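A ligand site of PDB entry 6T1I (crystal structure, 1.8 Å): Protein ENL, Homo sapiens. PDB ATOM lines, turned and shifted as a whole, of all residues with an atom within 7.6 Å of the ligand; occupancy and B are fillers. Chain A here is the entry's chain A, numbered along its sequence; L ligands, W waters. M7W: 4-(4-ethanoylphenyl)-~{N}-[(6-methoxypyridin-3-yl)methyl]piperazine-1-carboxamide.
N of Tyr 78 sits at hydrogen-bond distance from O1 of the ligand (2.9 Å).
N of the ligand lies within hydrogen-bond range of OG of Ser 58, at 3.0 Å.
The side-chain hydroxyl (OG) of Ser 58 sits at hydrogen-bond distance from a ring nitrogen (ND1) of His 56 (2.7 Å).
N of His 30 sits at hydrogen-bond distance from O of Gly 77 (2.9 Å).
N of Thr 29 is in hydrogen-bond range of O of Gly 77 (3.0 Å).
The backbone carbonyl oxygen of Pro 60 is in hydrogen-bond range of the guanidinium group of Arg 64.
Residues that only touch the ligand: Gly 77, Phe 28, Phe 59, Pro 60, Ala 79, His 56, Gly 80 and Ser 76.
Hydrophobic or aromatic side chains within 4 Å of the ligand: Phe 28, His 56, Phe 59, Pro 60, Tyr 78 and Ala 79.
Within 4 Å of the ligand: Phe 28, His 56, Ser 58, Phe 59, Pro 60, Ser 76, Gly 77, Tyr 78, Ala 79 and Gly 80.
Water W2 lies within hydrogen-bond range of an oxygen (O1) of the ligand (2.8 Å), the backbone carbonyl oxygen of Ala 79 (2.8 Å) and the indole nitrogen of Trp 32 (2.9 Å).
Water W1 lies within hydrogen-bond range of the backbone carbonyl oxygen of Ser 76 (2.5 Å) and the side-chain carboxylate of Glu 75 (2.7 Å).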
ATOM      1  N   GLU A  26      11.511  20.790  11.126  1.00  0.00           N
ATOM      2  CA  GLU A  26      11.967  20.904  12.529  1.00  0.00           C
ATOM      3  C   GLU A  26      12.970  22.063  12.647  1.00  0.00           C
ATOM      4  O   GLU A  26      13.415  22.354  13.804  1.00  0.00           O
ATOM      5  CB  GLU A  26      12.542  19.564  13.015  1.00  0.00           C
ATOM      6  CG  GLU A  26      11.461  18.556  13.389  1.00  0.00           C
ATOM      7  CD  GLU A  26      10.565  18.960  14.567  1.00  0.00           C
ATOM      8  OE1 GLU A  26      11.101  19.517  15.610  1.00  0.00           O
ATOM      9  OE2 GLU A  26       9.349  18.713  14.475  1.00  0.00           O
ATOM     10  N   GLY A  27      13.301  22.701  11.507  1.00  0.00           N
ATOM     11  CA  GLY A  27      14.359  23.734  11.417  1.00  0.00           C
ATOM     12  C   GLY A  27      15.782  23.150  11.438  1.00  0.00           C
ATOM     13  O   GLY A  27      16.745  23.867  11.865  1.00  0.00           O
ATOM     14  N   PHE A  28      15.957  21.895  11.021  1.00  0.00           N
ATOM     15  CA  PHE A  28      17.300  21.291  10.843  1.00  0.00           C
ATOM     16  C   PHE A  28      17.878  21.767   9.507  1.00  0.00           C
ATOM     17  O   PHE A  28      17.256  21.545   8.469  1.00  0.00           O
ATOM     18  CB  PHE A  28      17.247  19.772  10.925  1.00  0.00           C
ATOM     19  CG  PHE A  28      16.602  19.196  12.164  1.00  0.00           C
ATOM     20  CD1 PHE A  28      16.471  19.931  13.323  1.00  0.00           C
ATOM     21  CD2 PHE A  28      16.169  17.871  12.181  1.00  0.00           C
ATOM     22  CE1 PHE A  28      15.886  19.380  14.460  1.00  0.00           C
ATOM     23  CE2 PHE A  28      15.579  17.330  13.306  1.00  0.00           C
ATOM     24  CZ  PHE A  28      15.457  18.075  14.446  1.00  0.00           C
ATOM     25  N   THR A  29      18.984  22.482   9.581  1.00  0.00           N
ATOM     26  CA  THR A  29      19.614  23.231   8.473  1.00  0.00           C
ATOM     27  C   THR A  29      20.620  22.353   7.733  1.00  0.00           C
ATOM     28  O   THR A  29      20.862  22.601   6.521  1.00  0.00           O
ATOM     29  CB  THR A  29      20.269  24.489   9.042  1.00  0.00           C
ATOM     30  OG1 THR A  29      21.059  24.096  10.168  1.00  0.00           O
ATOM     31  CG2 THR A  29      19.233  25.516   9.474  1.00  0.00           C
ATOM     32  N   HIS A  30      21.206  21.358   8.429  1.00  0.00           N
ATOM     33  CA  HIS A  30      22.363  20.595   7.940  1.00  0.00           C
ATOM     34  C   HIS A  30      22.087  19.103   7.935  1.00  0.00           C
ATOM     35  O   HIS A  30      21.348  18.618   8.810  1.00  0.00           O
ATOM     36  CB  HIS A  30      23.630  20.877   8.770  1.00  0.00           C
ATOM     37  CG  HIS A  30      24.235  22.193   8.515  1.00  0.00           C
ATOM     38  ND1 HIS A  30      23.676  23.361   8.996  1.00  0.00           N
ATOM     39  CD2 HIS A  30      25.404  22.531   7.918  1.00  0.00           C
ATOM     40  CE1 HIS A  30      24.477  24.382   8.700  1.00  0.00           C
ATOM     41  NE2 HIS A  30      25.559  23.881   8.042  1.00  0.00           N
ATOM     42  N   TRP A  32      24.592  15.793   8.304  1.00  0.00           N
ATOM     43  CA  TRP A  32      25.971  15.431   8.700  1.00  0.00           C
ATOM     44  C   TRP A  32      26.091  13.932   8.907  1.00  0.00           C
ATOM     45  O   TRP A  32      25.072  13.204   9.015  1.00  0.00           O
ATOM     46  CB  TRP A  32      26.447  16.253   9.918  1.00  0.00           C
ATOM     47  CG  TRP A  32      25.625  16.149  11.165  1.00  0.00           C
ATOM     48  CD1 TRP A  32      24.825  17.131  11.716  1.00  0.00           C
ATOM     49  CD2 TRP A  32      25.684  15.079  12.116  1.00  0.00           C
ATOM     50  NE1 TRP A  32      24.345  16.705  12.928  1.00  0.00           N
ATOM     51  CE2 TRP A  32      24.838  15.428  13.178  1.00  0.00           C
ATOM     52  CE3 TRP A  32      26.350  13.836  12.147  1.00  0.00           C
ATOM     53  CZ2 TRP A  32      24.639  14.585  14.275  1.00  0.00           C
ATOM     54  CZ3 TRP A  32      26.119  12.993  13.200  1.00  0.00           C
ATOM     55  CH2 TRP A  32      25.332  13.398  14.288  1.00  0.00           C
ATOM     56  N   LEU A  55      25.988  11.339  21.033  1.00  0.00           N
ATOM     57  CA  LEU A  55      25.391  12.540  20.432  1.00  0.00           C
ATOM     58  C   LEU A  55      25.023  13.495  21.560  1.00  0.00           C
ATOM     59  O   LEU A  55      24.942  13.057  22.723  1.00  0.00           O
ATOM     60  CB  LEU A  55      24.163  12.155  19.620  1.00  0.00           C
ATOM     61  CG  LEU A  55      24.430  11.859  18.147  1.00  0.00           C
ATOM     62  CD1 LEU A  55      25.573  10.886  18.016  1.00  0.00           C
ATOM     63  CD2 LEU A  55      23.182  11.347  17.453  1.00  0.00           C
ATOM     64  N   HIS A  56      24.826  14.748  21.195  1.00  0.00           N
ATOM     65  CA  HIS A  56      24.405  15.835  22.109  1.00  0.00           C
ATOM     66  C   HIS A  56      23.093  15.403  22.819  1.00  0.00           C
ATOM     67  O   HIS A  56      22.257  14.760  22.167  1.00  0.00           O
ATOM     68  CB  HIS A  56      24.310  17.138  21.323  1.00  0.00           C
ATOM     69  CG  HIS A  56      24.193  18.329  22.201  1.00  0.00           C
ATOM     70  ND1 HIS A  56      22.990  18.864  22.513  1.00  0.00           N
ATOM     71  CD2 HIS A  56      25.120  19.002  22.907  1.00  0.00           C
ATOM     72  CE1 HIS A  56      23.158  19.892  23.327  1.00  0.00           C
ATOM     73  NE2 HIS A  56      24.449  19.973  23.613  1.00  0.00           N
ATOM     74  N   ASP A  57      22.934  15.763  24.114  1.00  0.00           N
ATOM     75  CA  ASP A  57      21.733  15.432  24.936  1.00  0.00           C
ATOM     76  C   ASP A  57      20.465  15.875  24.174  1.00  0.00           C
ATOM     77  O   ASP A  57      19.434  15.291  24.421  1.00  0.00           O
ATOM     78  CB  ASP A  57      21.788  16.094  26.325  1.00  0.00           C
ATOM     79  CG  ASP A  57      22.808  15.502  27.308  1.00  0.00           C
ATOM     80  OD1 ASP A  57      23.422  14.460  26.989  1.00  0.00           O
ATOM     81  OD2 ASP A  57      22.984  16.095  28.398  1.00  0.00           O
ATOM     82  N   SER A  58      20.570  16.784  23.196  1.00  0.00           N
ATOM     83  CA  SER A  58      19.420  17.343  22.426  1.00  0.00           C
ATOM     84  C   SER A  58      18.868  16.318  21.431  1.00  0.00           C
ATOM     85  O   SER A  58      17.735  16.522  20.906  1.00  0.00           O
ATOM     86  CB  SER A  58      19.785  18.654  21.740  1.00  0.00           C
ATOM     87  OG  SER A  58      20.910  18.523  20.851  1.00  0.00           O
ATOM     88  N   PHE A  59      19.593  15.224  21.185  1.00  0.00           N
ATOM     89  CA  PHE A  59      19.166  14.145  20.281  1.00  0.00           C
ATOM     90  C   PHE A  59      18.448  13.055  21.063  1.00  0.00           C
ATOM     91  O   PHE A  59      18.833  12.742  22.172  1.00  0.00           O
ATOM     92  CB  PHE A  59      20.360  13.535  19.556  1.00  0.00           C
ATOM     93  CG  PHE A  59      20.831  14.342  18.381  1.00  0.00           C
ATOM     94  CD1 PHE A  59      21.770  15.337  18.534  1.00  0.00           C
ATOM     95  CD2 PHE A  59      20.305  14.106  17.127  1.00  0.00           C
ATOM     96  CE1 PHE A  59      22.174  16.100  17.447  1.00  0.00           C
ATOM     97  CE2 PHE A  59      20.756  14.832  16.032  1.00  0.00           C
ATOM     98  CZ  PHE A  59      21.676  15.821  16.195  1.00  0.00           C
ATOM     99  N   PRO A  60      17.400  12.464  20.482  1.00  0.00           N
ATOM    100  CA  PRO A  60      16.786  11.268  21.063  1.00  0.00           C
ATOM    101  C   PRO A  60      17.735  10.073  20.973  1.00  0.00           C
ATOM    102  O   PRO A  60      18.459   9.977  19.990  1.00  0.00           O
ATOM    103  CB  PRO A  60      15.517  11.084  20.213  1.00  0.00           C
ATOM    104  CG  PRO A  60      15.919  11.655  18.862  1.00  0.00           C
ATOM    105  CD  PRO A  60      16.756  12.870  19.223  1.00  0.00           C
ATOM    106  N   ARG A  64      24.565   6.103  20.374  1.00  0.00           N
ATOM    107  CA  ARG A  64      24.406   5.359  19.101  1.00  0.00           C
ATOM    108  C   ARG A  64      25.498   4.317  19.024  1.00  0.00           C
ATOM    109  O   ARG A  64      26.647   4.683  19.083  1.00  0.00           O
ATOM    110  CB  ARG A  64      24.450   6.337  17.922  1.00  0.00           C
ATOM    111  CG  ARG A  64      23.420   7.463  18.046  1.00  0.00           C
ATOM    112  CD  ARG A  64      22.011   6.910  18.010  1.00  0.00           C
ATOM    113  NE  ARG A  64      21.038   7.966  18.134  1.00  0.00           N
ATOM    114  CZ  ARG A  64      20.644   8.751  17.145  1.00  0.00           C
ATOM    115  NH1 ARG A  64      19.791   9.733  17.390  1.00  0.00           N
ATOM    116  NH2 ARG A  64      21.120   8.569  15.932  1.00  0.00           N
ATOM    117  N   GLU A  75      22.816  12.122  10.490  1.00  0.00           N
ATOM    118  CA  GLU A  75      21.753  12.908  11.136  1.00  0.00           C
ATOM    119  C   GLU A  75      21.543  14.182  10.351  1.00  0.00           C
ATOM    120  O   GLU A  75      22.412  14.550   9.551  1.00  0.00           O
ATOM    121  CB  GLU A  75      22.102  13.222  12.586  1.00  0.00           C
ATOM    122  CG  GLU A  75      21.844  12.078  13.557  1.00  0.00           C
ATOM    123  CD  GLU A  75      20.397  11.619  13.641  1.00  0.00           C
ATOM    124  OE1 GLU A  75      19.495  12.438  13.383  1.00  0.00           O
ATOM    125  OE2 GLU A  75      20.179  10.427  13.932  1.00  0.00           O
ATOM    126  N   SER A  76      20.441  14.832  10.628  1.00  0.00           N
ATOM    127  CA  SER A  76      20.175  16.239  10.297  1.00  0.00           C
ATOM    128  C   SER A  76      20.114  17.034  11.588  1.00  0.00           C
ATOM    129  O   SER A  76      19.629  16.505  12.609  1.00  0.00           O
ATOM    130  CB  SER A  76      18.924  16.351   9.489  1.00  0.00           C
ATOM    131  OG  SER A  76      19.166  15.906   8.166  1.00  0.00           O
ATOM    132  N   GLY A  77      20.617  18.245  11.569  1.00  0.00           N
ATOM    133  CA  GLY A  77      20.605  19.095  12.764  1.00  0.00           C
ATOM    134  C   GLY A  77      20.886  20.534  12.422  1.00  0.00           C
ATOM    135  O   GLY A  77      20.858  20.896  11.228  1.00  0.00           O
ATOM    136  N   TYR A  78      21.115  21.339  13.443  1.00  0.00           N
ATOM    137  CA  TYR A  78      21.197  22.807  13.309  1.00  0.00           C
ATOM    138  C   TYR A  78      22.431  23.330  14.039  1.00  0.00           C
ATOM    139  O   TYR A  78      22.705  24.533  13.947  1.00  0.00           O
ATOM    140  CB  TYR A  78      19.889  23.422  13.785  1.00  0.00           C
ATOM    141  CG  TYR A  78      19.501  23.056  15.199  1.00  0.00           C
ATOM    142  CD1 TYR A  78      20.089  23.690  16.285  1.00  0.00           C
ATOM    143  CD2 TYR A  78      18.495  22.147  15.441  1.00  0.00           C
ATOM    144  CE1 TYR A  78      19.697  23.400  17.585  1.00  0.00           C
ATOM    145  CE2 TYR A  78      18.128  21.812  16.734  1.00  0.00           C
ATOM    146  CZ  TYR A  78      18.729  22.445  17.815  1.00  0.00           C
ATOM    147  OH  TYR A  78      18.361  22.137  19.100  1.00  0.00           O
ATOM    148  N   ALA A  79      23.212  22.473  14.710  1.00  0.00           N
ATOM    149  CA  ALA A  79      24.432  22.944  15.395  1.00  0.00           C
ATOM    150  C   ALA A  79      25.413  21.814  15.587  1.00  0.00           C
ATOM    151  O   ALA A  79      24.978  20.681  15.824  1.00  0.00           O
ATOM    152  CB  ALA A  79      24.100  23.608  16.729  1.00  0.00           C
ATOM    153  N   GLY A  80      26.687  22.157  15.545  1.00  0.00           N
ATOM    154  CA  GLY A  80      27.800  21.272  15.884  1.00  0.00           C
ATOM    155  C   GLY A  80      27.879  21.078  17.375  1.00  0.00           C
ATOM    156  O   GLY A  80      27.203  21.831  18.121  1.00  0.00           O
ATOM    157  N   PHE A  81      28.682  20.135  17.806  1.00  0.00           N
ATOM    158  CA  PHE A  81      28.905  19.849  19.234  1.00  0.00           C
ATOM    159  C   PHE A  81      30.150  19.002  19.324  1.00  0.00           C
ATOM    160  O   PHE A  81      30.574  18.445  18.302  1.00  0.00           O
ATOM    161  CB  PHE A  81      27.691  19.143  19.846  1.00  0.00           C
ATOM    162  CG  PHE A  81      27.180  17.956  19.069  1.00  0.00           C
ATOM    163  CD1 PHE A  81      26.258  18.128  18.048  1.00  0.00           C
ATOM    164  CD2 PHE A  81      27.586  16.661  19.373  1.00  0.00           C
ATOM    165  CE1 PHE A  81      25.749  17.050  17.358  1.00  0.00           C
ATOM    166  CE2 PHE A  81      27.067  15.573  18.679  1.00  0.00           C
ATOM    167  CZ  PHE A  81      26.149  15.774  17.681  1.00  0.00           C
ATOM    168  N   ILE A  82      30.632  18.804  20.548  1.00  0.00           N
ATOM    169  CA  ILE A  82      31.726  17.874  20.864  1.00  0.00           C
ATOM    170  C   ILE A  82      31.096  16.507  21.101  1.00  0.00           C
ATOM    171  O   ILE A  82      30.159  16.424  21.880  1.00  0.00           O
ATOM    172  CB  ILE A  82      32.496  18.379  22.098  1.00  0.00           C
ATOM    173  CG1 ILE A  82      33.071  19.764  21.855  1.00  0.00           C
ATOM    174  CG2 ILE A  82      33.577  17.389  22.485  1.00  0.00           C
ATOM    175  CD1 ILE A  82      34.036  19.820  20.689  1.00  0.00           C
ATOM    176  N   LEU A 104      32.452  17.797  16.060  1.00  0.00           N
ATOM    177  CA  LEU A 104      31.494  17.760  14.919  1.00  0.00           C
ATOM    178  C   LEU A 104      31.051  19.189  14.598  1.00  0.00           C
ATOM    179  O   LEU A 104      30.087  19.643  15.177  1.00  0.00           O
ATOM    180  CB  LEU A 104      30.291  16.902  15.272  1.00  0.00           C
ATOM    181  CG  LEU A 104      29.388  16.585  14.077  1.00  0.00           C
ATOM    182  CD1 LEU A 104      29.900  15.348  13.355  1.00  0.00           C
ATOM    183  CD2 LEU A 104      27.967  16.376  14.520  1.00  0.00           C
ATOM    184  N   LEU A 106      29.841  22.221  11.792  1.00  0.00           N
ATOM    185  CA  LEU A 106      29.056  22.389  10.557  1.00  0.00           C
ATOM    186  C   LEU A 106      29.616  23.575   9.786  1.00  0.00           C
ATOM    187  O   LEU A 106      30.345  24.357  10.380  1.00  0.00           O
ATOM    188  CB  LEU A 106      27.596  22.608  10.955  1.00  0.00           C
ATOM    189  CG  LEU A 106      26.989  21.535  11.844  1.00  0.00           C
ATOM    190  CD1 LEU A 106      25.524  21.858  12.119  1.00  0.00           C
ATOM    191  CD2 LEU A 106      27.133  20.153  11.210  1.00  0.00           C
HETATM  192  C2  M7W L   1      24.316  22.149  20.686  1.00  0.00           C
HETATM  193  C4  M7W L   1      22.765  21.017  19.259  1.00  0.00           C
HETATM  194  C5  M7W L   1      22.470  20.221  18.014  1.00  0.00           C
HETATM  195  C6  M7W L   1      20.578  19.252  16.878  1.00  0.00           C
HETATM  196  O2  M7W L   1      12.555  12.405  17.284  1.00  0.00           O
HETATM  197  C1  M7W L   1      23.233  22.645  21.380  1.00  0.00           C
HETATM  198  C3  M7W L   1      24.059  21.320  19.618  1.00  0.00           C
HETATM  199  O1  M7W L   1      20.993  19.646  15.795  1.00  0.00           O
HETATM  200  C13 M7W L   1      12.695  13.399  17.996  1.00  0.00           C
HETATM  201  C14 M7W L   1      11.778  13.644  19.145  1.00  0.00           C
HETATM  202  C12 M7W L   1      13.759  14.400  17.676  1.00  0.00           C
HETATM  203  C11 M7W L   1      13.809  15.618  18.340  1.00  0.00           C
HETATM  204  C10 M7W L   1      14.841  16.509  18.128  1.00  0.00           C
HETATM  205  C16 M7W L   1      14.784  14.085  16.789  1.00  0.00           C
HETATM  206  C15 M7W L   1      15.840  14.957  16.583  1.00  0.00           C
HETATM  207  C9  M7W L   1      15.894  16.179  17.256  1.00  0.00           C
HETATM  208  N2  M7W L   1      16.955  17.053  17.082  1.00  0.00           N
HETATM  209  C8  M7W L   1      17.342  17.980  18.155  1.00  0.00           C
HETATM  210  C7  M7W L   1      18.859  18.087  18.259  1.00  0.00           C
HETATM  211  C18 M7W L   1      18.043  16.749  16.142  1.00  0.00           C
HETATM  212  C17 M7W L   1      18.797  17.994  15.791  1.00  0.00           C
HETATM  213  N1  M7W L   1      19.417  18.566  16.986  1.00  0.00           N
HETATM  214  N   M7W L   1      21.211  19.486  18.055  1.00  0.00           N
HETATM  215  C19 M7W L   1      21.751  21.547  20.048  1.00  0.00           C
HETATM  216  N3  M7W L   1      21.969  22.352  21.096  1.00  0.00           N
HETATM  217  O   M7W L   1      23.526  23.487  22.384  1.00  0.00           O
HETATM  218  C   M7W L   1      22.448  24.011  23.146  1.00  0.00           C
HETATM  219  O   HOH W   1      18.106  14.705  13.439  1.00  0.00           O
HETATM  220  O   HOH W   2      23.387  18.598  14.931  1.00  0.00           O
